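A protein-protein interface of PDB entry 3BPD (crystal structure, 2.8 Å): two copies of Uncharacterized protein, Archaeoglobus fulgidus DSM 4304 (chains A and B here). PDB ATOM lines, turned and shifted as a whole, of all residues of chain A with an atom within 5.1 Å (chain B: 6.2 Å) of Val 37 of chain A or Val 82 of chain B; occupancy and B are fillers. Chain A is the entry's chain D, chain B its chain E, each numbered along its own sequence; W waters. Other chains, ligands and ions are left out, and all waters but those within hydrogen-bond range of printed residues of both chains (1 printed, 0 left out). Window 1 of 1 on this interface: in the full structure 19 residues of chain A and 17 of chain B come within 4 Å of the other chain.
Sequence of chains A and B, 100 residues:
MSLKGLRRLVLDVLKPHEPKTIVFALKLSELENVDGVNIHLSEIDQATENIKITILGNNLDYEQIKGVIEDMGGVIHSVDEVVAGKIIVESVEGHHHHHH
The backbone carbonyl oxygen (O) of Asp 35 of chain A sits at hydrogen-bond distance from the backbone NH (N) of Ile 87 of chain B, at 2.8 Å.
N of Val 37 of chain A sits at hydrogen-bond distance from O of Ala 84 of chain B, at 2.8 Å.
OE1 of Glu 81 of chain B lies within hydrogen-bond range of ND2 of Asn 38 of chain A (3.3 Å).
The side-chain amide nitrogen (ND2) of Asn 38 of chain A is in hydrogen-bond range of the backbone carbonyl oxygen (O) of Val 89 of chain B.
The backbone NH (N) of Ile 39 of chain A is in hydrogen-bond range of the backbone carbonyl oxygen (O) of Val 82 of chain B, 2.8 Å away.
The backbone NH of Thr 54 of chain A lies within hydrogen-bond range of the backbone carbonyl oxygen of Asn 38 of chain A (2.7 Å).
O of Val 83 of chain B sits at hydrogen-bond distance from N of Arg 7 of chain B.
The guanidinium group of Arg 7 of chain B sits close to the backbone carbonyl oxygen of Gly 85 of chain B (3.1 Å).
OE2 of Glu 81 of chain B lies within salt-bridge range of NH2 of Arg 8 of chain B.
The backbone carbonyl oxygen of Arg 8 of chain B lies within hydrogen-bond range of the backbone NH of Val 83 of chain B, 3.0 Å away.
The backbone NH (N) of Val 10 of chain B is in hydrogen-bond range of the backbone carbonyl oxygen (O) of Glu 81 of chain B.
Among the printed residues, merely in contact across the chains: Thr 21 of chain A with Val 82 of chain B (3.9 Å), Ile 22 of chain A with Val 82 of chain B (3.9 Å), Ala 25 of chain A with Val 82 of chain B (3.7 Å), Ala 25 of chain A with Ala 84 of chain B (3.98 Å), Ser 29 of chain A with Ala 84 of chain B (3.7 Å), Ser 29 of chain A with Gly 85 of chain B (3.8 Å), Asp 35 of chain A with Gly 85 of chain B (3.9 Å), Gly 36 of chain A with Ala 84 of chain B (3.4 Å), Gly 36 of chain A with Ile 87 of chain B (3.7 Å), Gly 36 of chain A with Val 89 of chain B (3.6 Å), Val 37 of chain A with Val 82 of chain B (3.8 Å), Val 37 of chain A with Val 83 of chain B (3.3 Å), Val 37 of chain A with Val 89 of chain B (3.97 Å), Asn 38 of chain A with Val 82 of chain B (3.4 Å), Asn 38 of chain A with Val 83 of chain B (3.6 Å), Ile 39 of chain A with Glu 81 of chain B (3.2 Å), Thr 54 of chain A with Val 89 of chain B (3.8 Å) and Leu 56 of chain A with Val 89 of chain B (3.9 Å).
Printed residues of chain B within 4 Å of Thr 21 of chain A: Val 82.
Val 37 of chain A touches four residues of chain B.
Val 79 of chain B touches none of the printed residues of chain A.
Of chain A, only Thr 21, Ile 22, Ala 25, Val 37, Asn 38 and Ile 39 come within 4 Å of Val 82 of chain B.
Of the printed residues of chain A, Gly 85 of chain B touches Ser 29 and Asp 35.
The nearest printed residue of chain A that does not touch Val 82 of chain B is Thr 54 of chain A (7.0 Å).
The nearest printed residue of chain A that does not touch Glu 81 of chain B is Thr 21 of chain A (6.4 Å).
Of the 14 printed residues of chain B, 7 touch a printed residue of chain A.
Of the 15 printed residues of chain A, 11 touch a printed residue of chain B.
Hydrophobic or aromatic side chains of chain A that line the printed part of chain B: Ile 22, Ala 25, Val 37 and Leu 56.
Among the printed residues, 23 pairs touch across the chains.
Among the printed residues, no Asp or Glu carboxylate lies within 4 Å of a Lys or Arg side-chain nitrogen of the other chain.
No position is printed for both chains.
Of the 23 pairs that touch across the chains among the printed residues, none has its exchanged pair printed and touching as well.
Water W1 bridges OG1 of Thr 21 of chain A (3.1 Å) and O of Val 79 of chain B (3.4 Å).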
ATOM      1  N   THR A  21      17.896 -20.107  13.409  1.00  0.00           N
ATOM      2  CA  THR A  21      17.814 -19.209  14.541  1.00  0.00           C
ATOM      3  C   THR A  21      16.425 -18.562  14.676  1.00  0.00           C
ATOM      4  O   THR A  21      16.055 -18.112  15.765  1.00  0.00           O
ATOM      5  CB  THR A  21      18.891 -18.121  14.444  1.00  0.00           C
ATOM      6  OG1 THR A  21      18.818 -17.486  13.163  1.00  0.00           O
ATOM      7  CG2 THR A  21      20.265 -18.728  14.619  1.00  0.00           C
ATOM      8  N   ILE A  22      15.649 -18.511  13.594  1.00  0.00           N
ATOM      9  CA  ILE A  22      14.317 -17.924  13.695  1.00  0.00           C
ATOM     10  C   ILE A  22      13.486 -18.847  14.565  1.00  0.00           C
ATOM     11  O   ILE A  22      12.554 -18.420  15.232  1.00  0.00           O
ATOM     12  CB  ILE A  22      13.604 -17.774  12.331  1.00  0.00           C
ATOM     13  CG1 ILE A  22      13.592 -19.103  11.594  1.00  0.00           C
ATOM     14  CG2 ILE A  22      14.280 -16.713  11.496  1.00  0.00           C
ATOM     15  CD1 ILE A  22      12.619 -19.116  10.428  1.00  0.00           C
ATOM     16  N   ALA A  25      14.601 -18.039  18.141  1.00  0.00           N
ATOM     17  CA  ALA A  25      13.971 -16.773  18.480  1.00  0.00           C
ATOM     18  C   ALA A  25      12.496 -16.934  18.828  1.00  0.00           C
ATOM     19  O   ALA A  25      12.045 -16.501  19.877  1.00  0.00           O
ATOM     20  CB  ALA A  25      14.129 -15.808  17.329  1.00  0.00           C
ATOM     21  N   LEU A  28      11.845 -19.064  22.201  1.00  0.00           N
ATOM     22  CA  LEU A  28      12.197 -18.234  23.348  1.00  0.00           C
ATOM     23  C   LEU A  28      11.190 -17.113  23.559  1.00  0.00           C
ATOM     24  O   LEU A  28      10.664 -16.942  24.659  1.00  0.00           O
ATOM     25  CB  LEU A  28      13.596 -17.655  23.180  1.00  0.00           C
ATOM     26  CG  LEU A  28      14.727 -18.663  23.399  1.00  0.00           C
ATOM     27  CD1 LEU A  28      15.995 -18.122  22.810  1.00  0.00           C
ATOM     28  CD2 LEU A  28      14.899 -18.960  24.874  1.00  0.00           C
ATOM     29  N   SER A  29      10.911 -16.359  22.504  1.00  0.00           N
ATOM     30  CA  SER A  29       9.949 -15.264  22.585  1.00  0.00           C
ATOM     31  C   SER A  29       8.569 -15.684  23.099  1.00  0.00           C
ATOM     32  O   SER A  29       7.805 -14.849  23.579  1.00  0.00           O
ATOM     33  CB  SER A  29       9.772 -14.621  21.210  1.00  0.00           C
ATOM     34  OG  SER A  29       9.156 -15.524  20.314  1.00  0.00           O
ATOM     35  N   VAL A  34       8.631 -13.259  28.931  1.00  0.00           N
ATOM     36  CA  VAL A  34       9.556 -12.672  27.967  1.00  0.00           C
ATOM     37  C   VAL A  34       8.957 -11.565  27.094  1.00  0.00           C
ATOM     38  O   VAL A  34       7.971 -11.781  26.379  1.00  0.00           O
ATOM     39  CB  VAL A  34      10.140 -13.792  27.064  1.00  0.00           C
ATOM     40  CG1 VAL A  34      10.894 -13.200  25.899  1.00  0.00           C
ATOM     41  CG2 VAL A  34      11.058 -14.690  27.882  1.00  0.00           C
ATOM     42  N   ASP A  35       9.571 -10.383  27.151  1.00  0.00           N
ATOM     43  CA  ASP A  35       9.127  -9.221  26.371  1.00  0.00           C
ATOM     44  C   ASP A  35       9.628  -9.261  24.927  1.00  0.00           C
ATOM     45  O   ASP A  35       8.921  -8.867  24.004  1.00  0.00           O
ATOM     46  CB  ASP A  35       9.625  -7.906  26.994  1.00  0.00           C
ATOM     47  CG  ASP A  35       8.977  -7.592  28.325  1.00  0.00           C
ATOM     48  OD1 ASP A  35       9.382  -8.189  29.342  1.00  0.00           O
ATOM     49  OD2 ASP A  35       8.058  -6.745  28.358  1.00  0.00           O
ATOM     50  N   GLY A  36      10.867  -9.708  24.751  1.00  0.00           N
ATOM     51  CA  GLY A  36      11.457  -9.778  23.429  1.00  0.00           C
ATOM     52  C   GLY A  36      12.764 -10.548  23.424  1.00  0.00           C
ATOM     53  O   GLY A  36      13.394 -10.743  24.460  1.00  0.00           O
ATOM     54  N   VAL A  37      13.176 -10.984  22.243  1.00  0.00           N
ATOM     55  CA  VAL A  37      14.395 -11.753  22.088  1.00  0.00           C
ATOM     56  C   VAL A  37      15.109 -11.264  20.853  1.00  0.00           C
ATOM     57  O   VAL A  37      14.480 -10.991  19.829  1.00  0.00           O
ATOM     58  CB  VAL A  37      14.076 -13.256  21.897  1.00  0.00           C
ATOM     59  CG1 VAL A  37      15.305 -13.997  21.400  1.00  0.00           C
ATOM     60  CG2 VAL A  37      13.566 -13.860  23.214  1.00  0.00           C
ATOM     61  N   ASN A  38      16.423 -11.130  20.958  1.00  0.00           N
ATOM     62  CA  ASN A  38      17.230 -10.713  19.817  1.00  0.00           C
ATOM     63  C   ASN A  38      18.342 -11.751  19.625  1.00  0.00           C
ATOM     64  O   ASN A  38      19.045 -12.128  20.578  1.00  0.00           O
ATOM     65  CB  ASN A  38      17.819  -9.307  20.044  1.00  0.00           C
ATOM     66  CG  ASN A  38      18.822  -8.899  18.962  1.00  0.00           C
ATOM     67  OD1 ASN A  38      19.878  -9.513  18.824  1.00  0.00           O
ATOM     68  ND2 ASN A  38      18.498  -7.860  18.200  1.00  0.00           N
ATOM     69  N   ILE A  39      18.467 -12.246  18.399  1.00  0.00           N
ATOM     70  CA  ILE A  39      19.504 -13.210  18.095  1.00  0.00           C
ATOM     71  C   ILE A  39      20.413 -12.584  17.055  1.00  0.00           C
ATOM     72  O   ILE A  39      19.969 -12.227  15.966  1.00  0.00           O
ATOM     73  CB  ILE A  39      18.916 -14.528  17.564  1.00  0.00           C
ATOM     74  CG1 ILE A  39      17.923 -15.081  18.592  1.00  0.00           C
ATOM     75  CG2 ILE A  39      20.043 -15.541  17.302  1.00  0.00           C
ATOM     76  CD1 ILE A  39      17.520 -16.517  18.362  1.00  0.00           C
ATOM     77  N   ILE A  53      22.398 -14.252  22.010  1.00  0.00           N
ATOM     78  CA  ILE A  53      20.982 -14.053  22.310  1.00  0.00           C
ATOM     79  C   ILE A  53      20.714 -13.033  23.429  1.00  0.00           C
ATOM     80  O   ILE A  53      21.238 -13.155  24.534  1.00  0.00           O
ATOM     81  CB  ILE A  53      20.334 -15.395  22.720  1.00  0.00           C
ATOM     82  CG1 ILE A  53      20.627 -16.454  21.655  1.00  0.00           C
ATOM     83  CG2 ILE A  53      18.823 -15.225  22.921  1.00  0.00           C
ATOM     84  CD1 ILE A  53      20.022 -17.823  21.960  1.00  0.00           C
ATOM     85  N   THR A  54      19.914 -12.013  23.129  1.00  0.00           N
ATOM     86  CA  THR A  54      19.549 -11.029  24.141  1.00  0.00           C
ATOM     87  C   THR A  54      18.072 -11.285  24.456  1.00  0.00           C
ATOM     88  O   THR A  54      17.223 -11.249  23.562  1.00  0.00           O
ATOM     89  CB  THR A  54      19.728  -9.583  23.643  1.00  0.00           C
ATOM     90  OG1 THR A  54      21.090  -9.370  23.265  1.00  0.00           O
ATOM     91  CG2 THR A  54      19.378  -8.595  24.753  1.00  0.00           C
ATOM     92  N   ILE A  55      17.788 -11.572  25.725  1.00  0.00           N
ATOM     93  CA  ILE A  55      16.435 -11.856  26.198  1.00  0.00           C
ATOM     94  C   ILE A  55      15.994 -10.823  27.224  1.00  0.00           C
ATOM     95  O   ILE A  55      16.643 -10.628  28.246  1.00  0.00           O
ATOM     96  CB  ILE A  55      16.348 -13.248  26.870  1.00  0.00           C
ATOM     97  CG1 ILE A  55      16.802 -14.335  25.902  1.00  0.00           C
ATOM     98  CG2 ILE A  55      14.919 -13.535  27.283  1.00  0.00           C
ATOM     99  CD1 ILE A  55      16.827 -15.712  26.523  1.00  0.00           C
ATOM    100  N   LEU A  56      14.878 -10.171  26.940  1.00  0.00           N
ATOM    101  CA  LEU A  56      14.311  -9.147  27.810  1.00  0.00           C
ATOM    102  C   LEU A  56      13.047  -9.694  28.445  1.00  0.00           C
ATOM    103  O   LEU A  56      12.216 -10.289  27.763  1.00  0.00           O
ATOM    104  CB  LEU A  56      13.943  -7.928  26.979  1.00  0.00           C
ATOM    105  CG  LEU A  56      13.529  -6.640  27.683  1.00  0.00           C
ATOM    106  CD1 LEU A  56      14.692  -6.086  28.494  1.00  0.00           C
ATOM    107  CD2 LEU A  56      13.096  -5.647  26.628  1.00  0.00           C
ATOM    108  N   LEU B   6       7.893 -13.103  14.800  1.00  0.00           N
ATOM    109  CA  LEU B   6       9.078 -12.486  14.218  1.00  0.00           C
ATOM    110  C   LEU B   6       8.779 -11.020  13.932  1.00  0.00           C
ATOM    111  O   LEU B   6       7.829 -10.701  13.219  1.00  0.00           O
ATOM    112  CB  LEU B   6       9.466 -13.193  12.923  1.00  0.00           C
ATOM    113  CG  LEU B   6      10.009 -14.621  13.000  1.00  0.00           C
ATOM    114  CD1 LEU B   6      10.317 -15.120  11.593  1.00  0.00           C
ATOM    115  CD2 LEU B   6      11.259 -14.659  13.870  1.00  0.00           C
ATOM    116  N   ARG B   7       9.609 -10.136  14.476  1.00  0.00           N
ATOM    117  CA  ARG B   7       9.426  -8.703  14.309  1.00  0.00           C
ATOM    118  C   ARG B   7      10.399  -8.038  13.339  1.00  0.00           C
ATOM    119  O   ARG B   7      10.035  -7.097  12.630  1.00  0.00           O
ATOM    120  CB  ARG B   7       9.515  -8.039  15.673  1.00  0.00           C
ATOM    121  CG  ARG B   7       8.640  -8.747  16.693  1.00  0.00           C
ATOM    122  CD  ARG B   7       7.156  -8.347  16.614  1.00  0.00           C
ATOM    123  NE  ARG B   7       6.882  -7.167  17.438  1.00  0.00           N
ATOM    124  CZ  ARG B   7       6.803  -5.928  16.970  1.00  0.00           C
ATOM    125  NH1 ARG B   7       6.967  -5.702  15.676  1.00  0.00           N
ATOM    126  NH2 ARG B   7       6.582  -4.918  17.797  1.00  0.00           N
ATOM    127  N   ARG B   8      11.637  -8.512  13.306  1.00  0.00           N
ATOM    128  CA  ARG B   8      12.621  -7.931  12.410  1.00  0.00           C
ATOM    129  C   ARG B   8      13.602  -8.999  11.954  1.00  0.00           C
ATOM    130  O   ARG B   8      13.982  -9.875  12.726  1.00  0.00           O
ATOM    131  CB  ARG B   8      13.361  -6.792  13.120  1.00  0.00           C
ATOM    132  CG  ARG B   8      14.077  -5.813  12.180  1.00  0.00           C
ATOM    133  CD  ARG B   8      14.615  -4.613  12.953  1.00  0.00           C
ATOM    134  NE  ARG B   8      15.738  -4.973  13.818  1.00  0.00           N
ATOM    135  CZ  ARG B   8      16.108  -4.282  14.889  1.00  0.00           C
ATOM    136  NH1 ARG B   8      15.443  -3.191  15.231  1.00  0.00           N
ATOM    137  NH2 ARG B   8      17.132  -4.690  15.625  1.00  0.00           N
ATOM    138  N   LEU B   9      14.000  -8.925  10.693  1.00  0.00           N
ATOM    139  CA  LEU B   9      14.945  -9.877  10.128  1.00  0.00           C
ATOM    140  C   LEU B   9      16.051  -9.122   9.402  1.00  0.00           C
ATOM    141  O   LEU B   9      15.761  -8.196   8.657  1.00  0.00           O
ATOM    142  CB  LEU B   9      14.246 -10.774   9.101  1.00  0.00           C
ATOM    143  CG  LEU B   9      13.129 -11.711   9.563  1.00  0.00           C
ATOM    144  CD1 LEU B   9      12.400 -12.313   8.368  1.00  0.00           C
ATOM    145  CD2 LEU B   9      13.733 -12.801  10.428  1.00  0.00           C
ATOM    146  N   VAL B  10      17.312  -9.462   9.639  1.00  0.00           N
ATOM    147  CA  VAL B  10      18.362  -8.822   8.851  1.00  0.00           C
ATOM    148  C   VAL B  10      18.883  -9.938   7.948  1.00  0.00           C
ATOM    149  O   VAL B  10      19.430 -10.944   8.409  1.00  0.00           O
ATOM    150  CB  VAL B  10      19.513  -8.242   9.683  1.00  0.00           C
ATOM    151  CG1 VAL B  10      20.508  -7.575   8.749  1.00  0.00           C
ATOM    152  CG2 VAL B  10      18.982  -7.213  10.669  1.00  0.00           C
ATOM    153  N   VAL B  79      21.049 -15.260   7.774  1.00  0.00           N
ATOM    154  CA  VAL B  79      20.128 -14.530   8.620  1.00  0.00           C
ATOM    155  C   VAL B  79      21.056 -13.923   9.662  1.00  0.00           C
ATOM    156  O   VAL B  79      21.531 -14.619  10.554  1.00  0.00           O
ATOM    157  CB  VAL B  79      19.139 -15.466   9.304  1.00  0.00           C
ATOM    158  CG1 VAL B  79      18.295 -14.685  10.298  1.00  0.00           C
ATOM    159  CG2 VAL B  79      18.259 -16.126   8.268  1.00  0.00           C
ATOM    160  N   ASP B  80      21.326 -12.630   9.549  1.00  0.00           N
ATOM    161  CA  ASP B  80      22.248 -11.994  10.470  1.00  0.00           C
ATOM    162  C   ASP B  80      21.678 -11.603  11.816  1.00  0.00           C
ATOM    163  O   ASP B  80      22.393 -11.599  12.820  1.00  0.00           O
ATOM    164  CB  ASP B  80      22.904 -10.813   9.777  1.00  0.00           C
ATOM    165  CG  ASP B  80      23.778 -11.255   8.621  1.00  0.00           C
ATOM    166  OD1 ASP B  80      23.980 -12.481   8.473  1.00  0.00           O
ATOM    167  OD2 ASP B  80      24.274 -10.396   7.861  1.00  0.00           O
ATOM    168  N   GLU B  81      20.393 -11.283  11.841  1.00  0.00           N
ATOM    169  CA  GLU B  81      19.746 -10.926  13.079  1.00  0.00           C
ATOM    170  C   GLU B  81      18.247 -11.162  13.032  1.00  0.00           C
ATOM    171  O   GLU B  81      17.586 -10.899  12.023  1.00  0.00           O
ATOM    172  CB  GLU B  81      20.020  -9.472  13.433  1.00  0.00           C
ATOM    173  CG  GLU B  81      19.336  -9.050  14.729  1.00  0.00           C
ATOM    174  CD  GLU B  81      19.534  -7.591  15.042  1.00  0.00           C
ATOM    175  OE1 GLU B  81      20.556  -7.248  15.686  1.00  0.00           O
ATOM    176  OE2 GLU B  81      18.670  -6.788  14.623  1.00  0.00           O
ATOM    177  N   VAL B  82      17.728 -11.671  14.144  1.00  0.00           N
ATOM    178  CA  VAL B  82      16.312 -11.943  14.285  1.00  0.00           C
ATOM    179  C   VAL B  82      15.827 -11.330  15.585  1.00  0.00           C
ATOM    180  O   VAL B  82      16.475 -11.447  16.628  1.00  0.00           O
ATOM    181  CB  VAL B  82      16.008 -13.447  14.370  1.00  0.00           C
ATOM    182  CG1 VAL B  82      14.497 -13.670  14.281  1.00  0.00           C
ATOM    183  CG2 VAL B  82      16.741 -14.198  13.289  1.00  0.00           C
ATOM    184  N   VAL B  83      14.682 -10.671  15.511  1.00  0.00           N
ATOM    185  CA  VAL B  83      14.082 -10.080  16.681  1.00  0.00           C
ATOM    186  C   VAL B  83      12.677 -10.637  16.732  1.00  0.00           C
ATOM    187  O   VAL B  83      11.946 -10.571  15.747  1.00  0.00           O
ATOM    188  CB  VAL B  83      14.012  -8.561  16.567  1.00  0.00           C
ATOM    189  CG1 VAL B  83      13.313  -7.977  17.799  1.00  0.00           C
ATOM    190  CG2 VAL B  83      15.411  -7.998  16.438  1.00  0.00           C
ATOM    191  N   ALA B  84      12.307 -11.217  17.863  1.00  0.00           N
ATOM    192  CA  ALA B  84      10.968 -11.761  18.003  1.00  0.00           C
ATOM    193  C   ALA B  84      10.411 -11.419  19.373  1.00  0.00           C
ATOM    194  O   ALA B  84      11.157 -11.249  20.340  1.00  0.00           O
ATOM    195  CB  ALA B  84      10.977 -13.271  17.803  1.00  0.00           C
ATOM    196  N   GLY B  85       9.090 -11.316  19.445  1.00  0.00           N
ATOM    197  CA  GLY B  85       8.441 -10.996  20.700  1.00  0.00           C
ATOM    198  C   GLY B  85       7.479  -9.842  20.545  1.00  0.00           C
ATOM    199  O   GLY B  85       7.046  -9.511  19.441  1.00  0.00           O
ATOM    200  N   ILE B  87       8.212  -6.781  22.236  1.00  0.00           N
ATOM    201  CA  ILE B  87       9.077  -5.603  22.243  1.00  0.00           C
ATOM    202  C   ILE B  87      10.267  -5.780  21.297  1.00  0.00           C
ATOM    203  O   ILE B  87      10.853  -6.863  21.226  1.00  0.00           O
ATOM    204  CB  ILE B  87       9.634  -5.331  23.658  1.00  0.00           C
ATOM    205  CG1 ILE B  87       8.521  -4.814  24.565  1.00  0.00           C
ATOM    206  CG2 ILE B  87      10.759  -4.321  23.598  1.00  0.00           C
ATOM    207  CD1 ILE B  87       9.030  -4.263  25.903  1.00  0.00           C
ATOM    208  N   VAL B  89      13.799  -5.799  20.615  1.00  0.00           N
ATOM    209  CA  VAL B  89      15.004  -5.781  21.434  1.00  0.00           C
ATOM    210  C   VAL B  89      16.241  -5.636  20.552  1.00  0.00           C
ATOM    211  O   VAL B  89      16.387  -6.334  19.561  1.00  0.00           O
ATOM    212  CB  VAL B  89      15.119  -7.069  22.267  1.00  0.00           C
ATOM    213  CG1 VAL B  89      16.393  -7.063  23.071  1.00  0.00           C
ATOM    214  CG2 VAL B  89      13.917  -7.195  23.182  1.00  0.00           C
HETATM  215  O   HOH W   1      21.443 -17.822  11.547  1.00  0.00           O
